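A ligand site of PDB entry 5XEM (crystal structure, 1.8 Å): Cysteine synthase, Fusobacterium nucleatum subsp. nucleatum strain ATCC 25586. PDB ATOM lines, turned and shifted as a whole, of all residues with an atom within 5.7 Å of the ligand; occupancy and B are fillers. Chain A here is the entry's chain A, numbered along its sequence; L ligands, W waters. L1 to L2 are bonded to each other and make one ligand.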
ATOM      1  N   THR A  45      -7.868 -16.394  25.029  1.00  0.00           N
ATOM      2  CA  THR A  45      -7.905 -16.106  23.609  1.00  0.00           C
ATOM      3  C   THR A  45      -8.299 -17.343  22.808  1.00  0.00           C
ATOM      4  O   THR A  45      -8.736 -17.199  21.652  1.00  0.00           O
ATOM      5  CB  THR A  45      -6.540 -15.567  23.106  1.00  0.00           C
ATOM      6  OG1 THR A  45      -6.732 -14.744  21.959  1.00  0.00           O
ATOM      7  CG2 THR A  45      -5.532 -16.693  22.768  1.00  0.00           C
ATOM      8  N   LYS A  46      -8.161 -18.525  23.388  1.00  0.00           N
ATOM      9  CA  LYS A  46      -8.395 -19.786  22.663  1.00  0.00           C
ATOM     10  C   LYS A  46      -9.851 -19.995  22.315  1.00  0.00           C
ATOM     11  O   LYS A  46     -10.158 -20.708  21.347  1.00  0.00           O
ATOM     12  CB  LYS A  46      -7.803 -21.000  23.400  1.00  0.00           C
ATOM     13  CG  LYS A  46      -6.294 -20.927  23.597  1.00  0.00           C
ATOM     14  CD  LYS A  46      -5.552 -20.713  22.286  1.00  0.00           C
ATOM     15  CE  LYS A  46      -4.146 -21.318  22.337  1.00  0.00           C
ATOM     16  NZ  LYS A  46      -3.541 -21.634  21.010  1.00  0.00           N
ATOM     17  N   ALA A  72      -5.625 -32.320  21.690  1.00  0.00           N
ATOM     18  CA  ALA A  72      -4.525 -32.183  22.646  1.00  0.00           C
ATOM     19  C   ALA A  72      -4.328 -30.711  23.037  1.00  0.00           C
ATOM     20  O   ALA A  72      -4.198 -29.822  22.175  1.00  0.00           O
ATOM     21  CB  ALA A  72      -3.238 -32.755  22.062  1.00  0.00           C
ATOM     22  N   THR A  73      -4.256 -30.466  24.340  1.00  0.00           N
ATOM     23  CA  THR A  73      -4.178 -29.096  24.818  1.00  0.00           C
ATOM     24  C   THR A  73      -3.418 -29.011  26.142  1.00  0.00           C
ATOM     25  O   THR A  73      -3.362 -29.993  26.883  1.00  0.00           O
ATOM     26  CB  THR A  73      -5.602 -28.516  24.999  1.00  0.00           C
ATOM     27  OG1 THR A  73      -5.532 -27.216  25.587  1.00  0.00           O
ATOM     28  CG2 THR A  73      -6.434 -29.385  25.882  1.00  0.00           C
ATOM     29  N   SER A  74      -2.858 -27.850  26.427  1.00  0.00           N
ATOM     30  CA  SER A  74      -2.308 -27.561  27.764  1.00  0.00           C
ATOM     31  C   SER A  74      -3.375 -27.055  28.717  1.00  0.00           C
ATOM     32  O   SER A  74      -3.121 -26.893  29.922  1.00  0.00           O
ATOM     33  CB  SER A  74      -1.161 -26.570  27.687  1.00  0.00           C
ATOM     34  OG  SER A  74      -1.616 -25.336  27.169  1.00  0.00           O
ATOM     35  N   GLY A  75      -4.556 -26.753  28.185  1.00  0.00           N
ATOM     36  CA  GLY A  75      -5.687 -26.377  28.996  1.00  0.00           C
ATOM     37  C   GLY A  75      -6.658 -25.432  28.303  1.00  0.00           C
ATOM     38  O   GLY A  75      -7.834 -25.733  28.174  1.00  0.00           O
ATOM     39  N   ASN A  76      -6.158 -24.268  27.887  1.00  0.00           N
ATOM     40  CA  ASN A  76      -7.043 -23.221  27.397  1.00  0.00           C
ATOM     41  C   ASN A  76      -7.790 -23.598  26.113  1.00  0.00           C
ATOM     42  O   ASN A  76      -8.976 -23.314  25.977  1.00  0.00           O
ATOM     43  CB  ASN A  76      -6.294 -21.919  27.228  1.00  0.00           C
ATOM     44  CG  ASN A  76      -6.131 -21.189  28.525  1.00  0.00           C
ATOM     45  OD1 ASN A  76      -7.014 -21.259  29.392  1.00  0.00           O
ATOM     46  ND2 ASN A  76      -4.986 -20.561  28.709  1.00  0.00           N
ATOM     47  N   THR A  77      -7.104 -24.220  25.149  1.00  0.00           N
ATOM     48  CA  THR A  77      -7.823 -24.664  23.938  1.00  0.00           C
ATOM     49  C   THR A  77      -8.918 -25.672  24.283  1.00  0.00           C
ATOM     50  O   THR A  77     -10.029 -25.614  23.736  1.00  0.00           O
ATOM     51  CB  THR A  77      -6.846 -25.168  22.873  1.00  0.00           C
ATOM     52  OG1 THR A  77      -5.987 -24.077  22.520  1.00  0.00           O
ATOM     53  CG2 THR A  77      -7.623 -25.639  21.618  1.00  0.00           C
ATOM     54  N   GLY A  78      -8.630 -26.554  25.241  1.00  0.00           N
ATOM     55  CA  GLY A  78      -9.625 -27.470  25.775  1.00  0.00           C
ATOM     56  C   GLY A  78     -10.807 -26.812  26.427  1.00  0.00           C
ATOM     57  O   GLY A  78     -11.961 -27.176  26.181  1.00  0.00           O
ATOM     58  N   ARG A 104      -7.544 -26.458  35.588  1.00  0.00           N
ATOM     59  CA  ARG A 104      -7.842 -26.752  34.177  1.00  0.00           C
ATOM     60  C   ARG A 104      -8.716 -27.998  34.010  1.00  0.00           C
ATOM     61  O   ARG A 104      -9.670 -27.963  33.241  1.00  0.00           O
ATOM     62  CB  ARG A 104      -6.536 -26.852  33.353  1.00  0.00           C
ATOM     63  CG  ARG A 104      -5.746 -25.547  33.226  1.00  0.00           C
ATOM     64  CD  ARG A 104      -4.395 -25.856  32.580  1.00  0.00           C
ATOM     65  NE  ARG A 104      -3.478 -24.740  32.299  1.00  0.00           N
ATOM     66  CZ  ARG A 104      -3.746 -23.688  31.508  1.00  0.00           C
ATOM     67  NH1 ARG A 104      -4.954 -23.559  30.951  1.00  0.00           N
ATOM     68  NH2 ARG A 104      -2.830 -22.767  31.286  1.00  0.00           N
ATOM     69  N   MET A 124       3.676 -31.897  25.216  1.00  0.00           N
ATOM     70  CA  MET A 124       2.503 -32.038  24.332  1.00  0.00           C
ATOM     71  C   MET A 124       2.647 -33.146  23.294  1.00  0.00           C
ATOM     72  O   MET A 124       1.665 -33.627  22.749  1.00  0.00           O
ATOM     73  CB  MET A 124       2.186 -30.719  23.620  1.00  0.00           C
ATOM     74  CG  MET A 124       1.779 -29.590  24.563  1.00  0.00           C
ATOM     75  SD  MET A 124       0.272 -29.997  25.500  1.00  0.00           S
ATOM     76  CE  MET A 124      -0.746 -30.470  24.141  1.00  0.00           C
ATOM     77  N   GLN A 146      -4.924 -27.529  16.871  1.00  0.00           N
ATOM     78  CA  GLN A 146      -4.417 -26.168  16.934  1.00  0.00           C
ATOM     79  C   GLN A 146      -2.974 -25.999  16.408  1.00  0.00           C
ATOM     80  O   GLN A 146      -2.580 -24.900  16.032  1.00  0.00           O
ATOM     81  CB  GLN A 146      -4.480 -25.658  18.368  1.00  0.00           C
ATOM     82  CG  GLN A 146      -3.684 -26.474  19.368  1.00  0.00           C
ATOM     83  CD  GLN A 146      -3.853 -25.954  20.775  1.00  0.00           C
ATOM     84  OE1 GLN A 146      -3.984 -24.751  20.990  1.00  0.00           O
ATOM     85  NE2 GLN A 146      -3.884 -26.866  21.719  1.00  0.00           N
ATOM     86  N   PHE A 147      -2.187 -27.081  16.436  1.00  0.00           N
ATOM     87  CA  PHE A 147      -0.793 -27.002  15.990  1.00  0.00           C
ATOM     88  C   PHE A 147      -0.626 -26.851  14.482  1.00  0.00           C
ATOM     89  O   PHE A 147       0.370 -26.281  14.033  1.00  0.00           O
ATOM     90  CB  PHE A 147      -0.024 -28.212  16.514  1.00  0.00           C
ATOM     91  CG  PHE A 147      -0.106 -28.345  17.987  1.00  0.00           C
ATOM     92  CD1 PHE A 147       0.695 -27.553  18.779  1.00  0.00           C
ATOM     93  CD2 PHE A 147      -1.038 -29.197  18.588  1.00  0.00           C
ATOM     94  CE1 PHE A 147       0.592 -27.623  20.164  1.00  0.00           C
ATOM     95  CE2 PHE A 147      -1.145 -29.255  19.967  1.00  0.00           C
ATOM     96  CZ  PHE A 147      -0.328 -28.473  20.744  1.00  0.00           C
ATOM     97  N   ASN A 152      -6.536 -21.516  13.299  1.00  0.00           N
ATOM     98  CA  ASN A 152      -5.938 -20.896  14.493  1.00  0.00           C
ATOM     99  C   ASN A 152      -5.402 -19.483  14.162  1.00  0.00           C
ATOM    100  O   ASN A 152      -6.015 -18.462  14.540  1.00  0.00           O
ATOM    101  CB  ASN A 152      -4.945 -21.906  15.126  1.00  0.00           C
ATOM    102  CG  ASN A 152      -4.055 -21.333  16.187  1.00  0.00           C
ATOM    103  OD1 ASN A 152      -4.078 -20.125  16.500  1.00  0.00           O
ATOM    104  ND2 ASN A 152      -3.215 -22.210  16.744  1.00  0.00           N
ATOM    105  N   HIS A 156      -7.218 -14.986  14.511  1.00  0.00           N
ATOM    106  CA  HIS A 156      -6.545 -13.789  15.045  1.00  0.00           C
ATOM    107  C   HIS A 156      -6.269 -12.767  13.949  1.00  0.00           C
ATOM    108  O   HIS A 156      -6.334 -11.559  14.178  1.00  0.00           O
ATOM    109  CB  HIS A 156      -5.238 -14.181  15.719  1.00  0.00           C
ATOM    110  CG  HIS A 156      -5.429 -15.079  16.934  1.00  0.00           C
ATOM    111  ND1 HIS A 156      -5.998 -14.631  18.078  1.00  0.00           N
ATOM    112  CD2 HIS A 156      -5.138 -16.414  17.142  1.00  0.00           C
ATOM    113  CE1 HIS A 156      -6.059 -15.650  18.981  1.00  0.00           C
ATOM    114  NE2 HIS A 156      -5.494 -16.739  18.408  1.00  0.00           N
ATOM    115  N   GLY A 178       3.031 -13.831  23.485  1.00  0.00           N
ATOM    116  CA  GLY A 178       3.591 -15.085  23.916  1.00  0.00           C
ATOM    117  C   GLY A 178       3.291 -16.178  22.917  1.00  0.00           C
ATOM    118  O   GLY A 178       2.310 -16.081  22.187  1.00  0.00           O
ATOM    119  N   THR A 179       4.119 -17.216  22.877  1.00  0.00           N
ATOM    120  CA  THR A 179       3.934 -18.325  21.933  1.00  0.00           C
ATOM    121  C   THR A 179       3.862 -19.700  22.595  1.00  0.00           C
ATOM    122  O   THR A 179       4.553 -19.977  23.593  1.00  0.00           O
ATOM    123  CB  THR A 179       5.063 -18.379  20.851  1.00  0.00           C
ATOM    124  OG1 THR A 179       6.348 -18.613  21.492  1.00  0.00           O
ATOM    125  CG2 THR A 179       5.076 -17.077  20.072  1.00  0.00           C
ATOM    126  N   GLY A 180       3.026 -20.539  22.006  1.00  0.00           N
ATOM    127  CA  GLY A 180       2.925 -21.960  22.283  1.00  0.00           C
ATOM    128  C   GLY A 180       2.729 -22.664  20.946  1.00  0.00           C
ATOM    129  O   GLY A 180       3.656 -23.310  20.418  1.00  0.00           O
ATOM    130  N   THR A 181       1.537 -22.562  20.360  1.00  0.00           N
ATOM    131  CA  THR A 181       1.361 -22.944  18.957  1.00  0.00           C
ATOM    132  C   THR A 181       2.030 -21.918  18.000  1.00  0.00           C
ATOM    133  O   THR A 181       2.559 -22.290  16.946  1.00  0.00           O
ATOM    134  CB  THR A 181      -0.123 -23.084  18.522  1.00  0.00           C
ATOM    135  OG1 THR A 181      -0.745 -21.805  18.448  1.00  0.00           O
ATOM    136  CG2 THR A 181      -0.895 -24.059  19.405  1.00  0.00           C
ATOM    137  N   GLY A 182       2.025 -20.659  18.416  1.00  0.00           N
ATOM    138  CA  GLY A 182       2.513 -19.538  17.657  1.00  0.00           C
ATOM    139  C   GLY A 182       1.416 -18.880  16.849  1.00  0.00           C
ATOM    140  O   GLY A 182       1.673 -17.940  16.067  1.00  0.00           O
ATOM    141  N   GLY A 183       0.211 -19.377  17.013  1.00  0.00           N
ATOM    142  CA  GLY A 183      -0.914 -18.927  16.192  1.00  0.00           C
ATOM    143  C   GLY A 183      -1.384 -17.551  16.505  1.00  0.00           C
ATOM    144  O   GLY A 183      -1.665 -16.764  15.584  1.00  0.00           O
ATOM    145  N   SER A 184      -1.528 -17.209  17.781  1.00  0.00           N
ATOM    146  CA  SER A 184      -1.958 -15.846  18.107  1.00  0.00           C
ATOM    147  C   SER A 184      -0.913 -14.832  17.649  1.00  0.00           C
ATOM    148  O   SER A 184      -1.277 -13.792  17.070  1.00  0.00           O
ATOM    149  CB  SER A 184      -2.314 -15.677  19.600  1.00  0.00           C
ATOM    150  OG  SER A 184      -1.234 -16.068  20.404  1.00  0.00           O
ATOM    151  N   PHE A 185       0.373 -15.107  17.912  1.00  0.00           N
ATOM    152  CA  PHE A 185       1.408 -14.221  17.390  1.00  0.00           C
ATOM    153  C   PHE A 185       1.314 -14.088  15.869  1.00  0.00           C
ATOM    154  O   PHE A 185       1.335 -12.962  15.306  1.00  0.00           O
ATOM    155  CB  PHE A 185       2.817 -14.723  17.745  1.00  0.00           C
ATOM    156  CG  PHE A 185       3.889 -14.024  16.956  1.00  0.00           C
ATOM    157  CD1 PHE A 185       4.197 -12.697  17.239  1.00  0.00           C
ATOM    158  CD2 PHE A 185       4.500 -14.639  15.894  1.00  0.00           C
ATOM    159  CE1 PHE A 185       5.105 -12.003  16.465  1.00  0.00           C
ATOM    160  CE2 PHE A 185       5.441 -13.951  15.120  1.00  0.00           C
ATOM    161  CZ  PHE A 185       5.729 -12.636  15.409  1.00  0.00           C
ATOM    162  N   HIS A 220       9.893 -25.517  31.916  1.00  0.00           N
ATOM    163  CA  HIS A 220       9.550 -24.140  32.278  1.00  0.00           C
ATOM    164  C   HIS A 220       8.196 -24.146  32.947  1.00  0.00           C
ATOM    165  O   HIS A 220       7.461 -25.139  32.873  1.00  0.00           O
ATOM    166  CB  HIS A 220       9.542 -23.228  31.043  1.00  0.00           C
ATOM    167  CG  HIS A 220       8.375 -23.493  30.123  1.00  0.00           C
ATOM    168  ND1 HIS A 220       7.196 -22.827  30.251  1.00  0.00           N
ATOM    169  CD2 HIS A 220       8.215 -24.388  29.065  1.00  0.00           C
ATOM    170  CE1 HIS A 220       6.320 -23.322  29.343  1.00  0.00           C
ATOM    171  NE2 HIS A 220       6.939 -24.258  28.616  1.00  0.00           N
ATOM    172  N   GLN A 223       2.984 -21.599  31.995  1.00  0.00           N
ATOM    173  CA  GLN A 223       1.936 -22.479  31.462  1.00  0.00           C
ATOM    174  C   GLN A 223       1.274 -21.940  30.218  1.00  0.00           C
ATOM    175  O   GLN A 223       0.863 -20.781  30.178  1.00  0.00           O
ATOM    176  CB  GLN A 223       0.884 -22.763  32.552  1.00  0.00           C
ATOM    177  CG  GLN A 223       1.430 -23.462  33.774  1.00  0.00           C
ATOM    178  CD  GLN A 223       0.340 -23.844  34.780  1.00  0.00           C
ATOM    179  OE1 GLN A 223      -0.759 -24.309  34.386  1.00  0.00           O
ATOM    180  NE2 GLN A 223       0.635 -23.682  36.069  1.00  0.00           N
ATOM    181  N   GLY A 224       1.132 -22.796  29.190  1.00  0.00           N
ATOM    182  CA  GLY A 224       0.549 -22.382  27.909  1.00  0.00           C
ATOM    183  C   GLY A 224       1.607 -21.993  26.890  1.00  0.00           C
ATOM    184  O   GLY A 224       1.454 -22.219  25.659  1.00  0.00           O
ATOM    185  N   MET A 225       2.708 -21.428  27.361  1.00  0.00           N
ATOM    186  CA  MET A 225       3.781 -21.073  26.410  1.00  0.00           C
ATOM    187  C   MET A 225       4.741 -22.261  26.253  1.00  0.00           C
ATOM    188  O   MET A 225       4.617 -23.284  26.936  1.00  0.00           O
ATOM    189  CB  MET A 225       4.495 -19.814  26.876  1.00  0.00           C
ATOM    190  CG  MET A 225       3.804 -18.535  26.434  1.00  0.00           C
ATOM    191  SD  MET A 225       4.442 -17.025  27.171  1.00  0.00           S
ATOM    192  CE  MET A 225       6.179 -17.148  26.632  1.00  0.00           C
ATOM    193  N   GLY A 226       5.699 -22.121  25.347  1.00  0.00           N
ATOM    194  CA  GLY A 226       6.680 -23.152  25.078  1.00  0.00           C
ATOM    195  C   GLY A 226       6.189 -24.093  23.985  1.00  0.00           C
ATOM    196  O   GLY A 226       4.998 -24.184  23.727  1.00  0.00           O
ATOM    197  N   MET A 227       7.127 -24.786  23.376  1.00  0.00           N
ATOM    198  CA  MET A 227       6.869 -25.656  22.221  1.00  0.00           C
ATOM    199  C   MET A 227       7.394 -27.035  22.530  1.00  0.00           C
ATOM    200  O   MET A 227       8.604 -27.241  22.529  1.00  0.00           O
ATOM    201  CB  MET A 227       7.604 -25.085  21.023  1.00  0.00           C
ATOM    202  CG  MET A 227       6.879 -23.863  20.479  1.00  0.00           C
ATOM    203  SD  MET A 227       7.804 -23.021  19.169  1.00  0.00           S
ATOM    204  CE  MET A 227       6.753 -21.602  18.873  1.00  0.00           C
ATOM    205  N   SER A 228       6.495 -27.972  22.821  1.00  0.00           N
ATOM    206  CA  SER A 228       6.899 -29.322  23.261  1.00  0.00           C
ATOM    207  C   SER A 228       6.310 -30.470  22.454  1.00  0.00           C
ATOM    208  O   SER A 228       6.240 -31.627  22.959  1.00  0.00           O
ATOM    209  CB  SER A 228       6.616 -29.513  24.768  1.00  0.00           C
ATOM    210  OG  SER A 228       5.235 -29.481  25.100  1.00  0.00           O
ATOM    211  N   ILE A 229       5.890 -30.195  21.234  1.00  0.00           N
ATOM    212  CA  ILE A 229       5.367 -31.281  20.358  1.00  0.00           C
ATOM    213  C   ILE A 229       6.478 -31.994  19.570  1.00  0.00           C
ATOM    214  O   ILE A 229       6.170 -32.911  18.816  1.00  0.00           O
ATOM    215  CB  ILE A 229       4.253 -30.821  19.375  1.00  0.00           C
ATOM    216  CG1 ILE A 229       4.809 -29.921  18.248  1.00  0.00           C
ATOM    217  CG2 ILE A 229       3.142 -30.124  20.149  1.00  0.00           C
ATOM    218  CD1 ILE A 229       3.819 -29.622  17.120  1.00  0.00           C
ATOM    219  N   SER A 270       1.620 -16.557  31.544  1.00  0.00           N
ATOM    220  CA  SER A 270       2.108 -16.098  30.243  1.00  0.00           C
ATOM    221  C   SER A 270       1.912 -14.613  30.022  1.00  0.00           C
ATOM    222  O   SER A 270       2.668 -13.992  29.252  1.00  0.00           O
ATOM    223  CB  SER A 270       1.524 -16.923  29.079  1.00  0.00           C
ATOM    224  OG  SER A 270       0.195 -16.570  28.771  1.00  0.00           O
ATOM    225  N   THR A 297      -2.987 -13.494  27.147  1.00  0.00           N
ATOM    226  CA  THR A 297      -3.660 -14.672  26.586  1.00  0.00           C
ATOM    227  C   THR A 297      -4.810 -15.178  27.457  1.00  0.00           C
ATOM    228  O   THR A 297      -5.856 -15.579  26.932  1.00  0.00           O
ATOM    229  CB  THR A 297      -2.664 -15.802  26.311  1.00  0.00           C
ATOM    230  OG1 THR A 297      -1.682 -15.319  25.376  1.00  0.00           O
ATOM    231  CG2 THR A 297      -3.390 -17.019  25.727  1.00  0.00           C
ATOM    232  N   ASP A 298      -4.638 -15.138  28.783  1.00  0.00           N
ATOM    233  CA  ASP A 298      -5.693 -15.601  29.678  1.00  0.00           C
ATOM    234  C   ASP A 298      -5.730 -14.857  30.984  1.00  0.00           C
ATOM    235  O   ASP A 298      -4.783 -14.156  31.337  1.00  0.00           O
ATOM    236  CB  ASP A 298      -5.714 -17.144  29.862  1.00  0.00           C
ATOM    237  CG  ASP A 298      -4.655 -17.694  30.791  1.00  0.00           C
ATOM    238  OD1 ASP A 298      -3.676 -16.978  31.102  1.00  0.00           O
ATOM    239  OD2 ASP A 298      -4.785 -18.889  31.166  1.00  0.00           O
ATOM    240  N   TYR A 303      -4.668 -20.036  38.032  1.00  0.00           N
ATOM    241  CA  TYR A 303      -3.307 -20.307  38.507  1.00  0.00           C
ATOM    242  C   TYR A 303      -3.193 -20.051  40.009  1.00  0.00           C
ATOM    243  O   TYR A 303      -2.228 -20.436  40.630  1.00  0.00           O
ATOM    244  CB  TYR A 303      -2.302 -19.415  37.795  1.00  0.00           C
ATOM    245  CG  TYR A 303      -2.411 -19.562  36.306  1.00  0.00           C
ATOM    246  CD1 TYR A 303      -1.846 -20.648  35.677  1.00  0.00           C
ATOM    247  CD2 TYR A 303      -3.110 -18.644  35.517  1.00  0.00           C
ATOM    248  CE1 TYR A 303      -1.988 -20.830  34.300  1.00  0.00           C
ATOM    249  CE2 TYR A 303      -3.214 -18.808  34.133  1.00  0.00           C
ATOM    250  CZ  TYR A 303      -2.661 -19.914  33.538  1.00  0.00           C
ATOM    251  OH  TYR A 303      -2.762 -20.126  32.173  1.00  0.00           O
HETATM  252  N1  LIG L   1      -1.927 -22.723  24.941  1.00  0.00           N
HETATM  253  C1  LIG L   1      -2.239 -23.914  24.128  1.00  0.00           C
HETATM  254  C2  LIG L   1      -1.010 -24.857  24.062  1.00  0.00           C
HETATM  255  S1  LIG L   1       0.341 -24.220  23.090  1.00  0.00           S
HETATM  256  C3  LIG L   1       1.587 -25.517  23.052  1.00  0.00           C
HETATM  257  C4  LIG L   1       2.162 -25.915  24.447  1.00  0.00           C
HETATM  258  N2  LIG L   1       2.583 -24.739  25.208  1.00  0.00           N
HETATM  259  C5  LIG L   1       3.398 -26.818  24.198  1.00  0.00           C
HETATM  260  O1  LIG L   1       4.102 -27.079  25.218  1.00  0.00           O
HETATM  261  O2  LIG L   1       3.668 -27.249  23.037  1.00  0.00           O
HETATM  262  C6  LIG L   1      -3.431 -24.661  24.681  1.00  0.00           C
HETATM  263  O3  LIG L   1      -4.238 -24.015  25.371  1.00  0.00           O
HETATM  264  O4  LIG L   1      -3.546 -25.872  24.369  1.00  0.00           O
HETATM  265  N1  LG2 L   2      -0.626 -18.348  27.056  1.00  0.00           N
HETATM  266  C1  LG2 L   2      -1.516 -19.280  27.446  1.00  0.00           C
HETATM  267  C2  LG2 L   2      -2.143 -19.188  28.838  1.00  0.00           C
HETATM  268  C3  LG2 L   2      -1.887 -20.329  26.593  1.00  0.00           C
HETATM  269  O1  LG2 L   2      -2.805 -21.250  27.006  1.00  0.00           O
HETATM  270  C4  LG2 L   2      -1.332 -20.428  25.329  1.00  0.00           C
HETATM  271  C5  LG2 L   2      -1.710 -21.546  24.365  1.00  0.00           C
HETATM  272  C6  LG2 L   2      -0.413 -19.440  24.948  1.00  0.00           C
HETATM  273  C7  LG2 L   2      -0.095 -18.415  25.836  1.00  0.00           C
HETATM  274  C8  LG2 L   2       0.257 -19.425  23.591  1.00  0.00           C
HETATM  275  O2  LG2 L   2      -0.720 -19.060  22.544  1.00  0.00           O
HETATM  276  P1  LG2 L   2      -0.605 -19.578  21.017  1.00  0.00           P
HETATM  277  O3  LG2 L   2      -1.535 -18.858  20.204  1.00  0.00           O
HETATM  278  O4  LG2 L   2      -0.842 -21.003  21.104  1.00  0.00           O
HETATM  279  O5  LG2 L   2       0.819 -19.361  20.671  1.00  0.00           O
HETATM  280  O   HOH W   1      -3.220 -23.532  28.488  1.00  0.00           O
HETATM  281  O   HOH W   2      -4.091 -19.232  19.260  1.00  0.00           O
HETATM  282  O   HOH W   3       3.784 -26.168  20.402  1.00  0.00           O
HETATM  283  O   HOH W   4       6.436 -26.247  26.680  1.00  0.00           O
HETATM  284  O   HOH W   5       1.556 -17.001  19.546  1.00  0.00           O
HETATM  285  O   HOH W   6      -1.891 -16.254  22.963  1.00  0.00           O
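The side-chain hydroxyl (OG) of Ser 270 sits at hydrogen-bond distance from a nitrogen (N1) of LG2 L2, at 2.6 Å. The backbone NH (N) of Ser 228 lies within hydrogen-bond range of an oxygen (O2) of LIG L1 (2.9 Å). An oxygen (O1) of LIG L1 sits at hydrogen-bond distance from the side-chain hydroxyl (OG) of Ser 228 (2.7 Å). An oxygen (O4) of LIG L1 sits at hydrogen-bond distance from the side-chain hydroxyl of Thr 73 (2.7 Å). An oxygen (O4) of LG2 L2 lies within salt-bridge range of the side-chain amino group (NZ) of Lys 46, at 2.8 Å. The backbone NH of Thr 181 lies within hydrogen-bond range of an oxygen (O4) of LG2 L2, 2.9 Å away. The side-chain hydroxyl of Thr 181 sits at hydrogen-bond distance from an oxygen (O4) of LG2 L2 (2.8 Å). O of Gly 224 lies within hydrogen-bond range of N2 of LIG L1. N of Ser 184 sits at hydrogen-bond distance from O3 of LG2 L2 (2.9 Å). The side-chain hydroxyl (OG) of Ser 184 lies within hydrogen-bond range of an oxygen (O3) of LG2 L2 (2.8 Å). The backbone NH (N) of Gly 180 sits at hydrogen-bond distance from an oxygen (O5) of LG2 L2, 2.8 Å away. The side-chain amide nitrogen (NE2) of Gln 146 sits at hydrogen-bond distance from an oxygen (O4) of LIG L1 (2.9 Å). The backbone NH of Asn 76 is in hydrogen-bond range of an oxygen (O3) of LIG L1, 3.2 Å away. ND2 of Asn 76 sits at hydrogen-bond distance from O1 of LG2 L2 (2.9 Å). N of Gly 182 lies within hydrogen-bond range of O5 of LG2 L2, 2.9 Å away. N of Thr 77 is in hydrogen-bond range of O3 of LIG L1. OG1 of Thr 77 sits at hydrogen-bond distance from O3 of LIG L1. N2 of LIG L1 is in hydrogen-bond range of O of Gly 226, 2.9 Å away. The backbone NH (N) of Ser 74 sits at hydrogen-bond distance from an oxygen (O4) of LIG L1, at 2.9 Å. The side-chain hydroxyl of Ser 74 lies close to an oxygen (O3) of LIG L1. A nitrogen (N2) of LIG L1 sits at hydrogen-bond distance from the backbone carbonyl oxygen (O) of Met 225 (3.0 Å).
OG1 of Thr 73 sits at hydrogen-bond distance from N of Gly 75, at 2.8 Å. The side-chain hydroxyl (OG1) of Thr 181 lies within hydrogen-bond range of the backbone NH (N) of Gly 183, at 3.0 Å. The side-chain hydroxyl of Thr 77 lies within hydrogen-bond range of the side-chain amide oxygen of Gln 146, at 2.6 Å. NE2 of Gln 146 is in hydrogen-bond range of O of Ala 72 (3.0 Å). The side-chain amide nitrogen of Asn 76 sits at hydrogen-bond distance from the side-chain carboxylate of Asp 298 (3.0 Å). The backbone carbonyl oxygen of Ser 74 sits close to the guanidinium group of Arg 104 (3.2 Å). The backbone carbonyl oxygen of Met 225 lies close to a ring nitrogen (NE2) of His 220 (3.0 Å). OH of Tyr 303 lies within hydrogen-bond range of NH2 of Arg 104.
N of Gly 75 touches O3 of LIG L1, at 3.9 Å. CG of Met 124 touches C5 of LIG L1 (3.2 Å). CE1 of Phe 147 touches C3 of LIG L1, at 3.7 Å. O of Gly 178 touches O5 of LG2 L2 (3.9 Å). CA of Thr 179 touches O5 of LG2 L2, at 3.5 Å. Gly 183 touches the ligand. O of Gln 223 touches C2 of LG2 L2 (3.7 Å). CA of Met 227 touches O2 of LIG L1 (3.7 Å). CG2 of Thr 297 touches N1 of LG2 L2, 3.3 Å away. CG of Asp 298 touches C2 of LG2 L2, at 3.5 Å. Tyr 303 touches the ligand. Hydrophobic or aromatic side chains within 4 Å of the ligand: Met 124, Phe 147 and Met 225. Within 4 Å of the ligand: Lys 46, Thr 73, Ser 74, Gly 75, Asn 76, Thr 77, Met 124, Gln 146, Phe 147, Gly 178, Thr 179, Gly 180, Thr 181, Gly 182, Gly 183, Ser 184, Gln 223, Gly 224, Met 225, Gly 226, Met 227, Ser 228, Ser 270, Thr 297, Asp 298 and Tyr 303. The nearest printed residue that does not touch the ligand is Ile 229 (4.1 Å).
Water W5 lies within hydrogen-bond range of O5 of LG2 L2 (2.7 Å), N of Phe 185 (2.8 Å), O of Gly 178 (2.9 Å) and OG of Ser 184 (3.1 Å). Water W2 lies within hydrogen-bond range of an oxygen (O3) of LG2 L2 (2.8 Å), the side-chain amide oxygen (OD1) of Asn 152 (2.9 Å), a ring nitrogen (NE2) of His 156 (3.0 Å) and the side-chain amino group (NZ) of Lys 46 (3.0 Å). Water W1 lies within hydrogen-bond range of the side-chain hydroxyl of Ser 74 (2.8 Å), an oxygen (O1) of LG2 L2 (2.8 Å), the guanidinium group of Arg 104 (2.9 Å) and the backbone NH of Asn 76 (3.1 Å). Water W3 lies within hydrogen-bond range of an oxygen (O2) of LIG L1 and the backbone carbonyl oxygen (O) of Gly 180. Water W4 lies within hydrogen-bond range of a ring nitrogen (NE2) of His 220 (2.8 Å), an oxygen (O1) of LIG L1 (2.9 Å) and the backbone carbonyl oxygen of Met 225 (3.5 Å). Water W6 lies within hydrogen-bond range of OG1 of Thr 297, OG of Ser 184 and O2 of LG2 L2.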
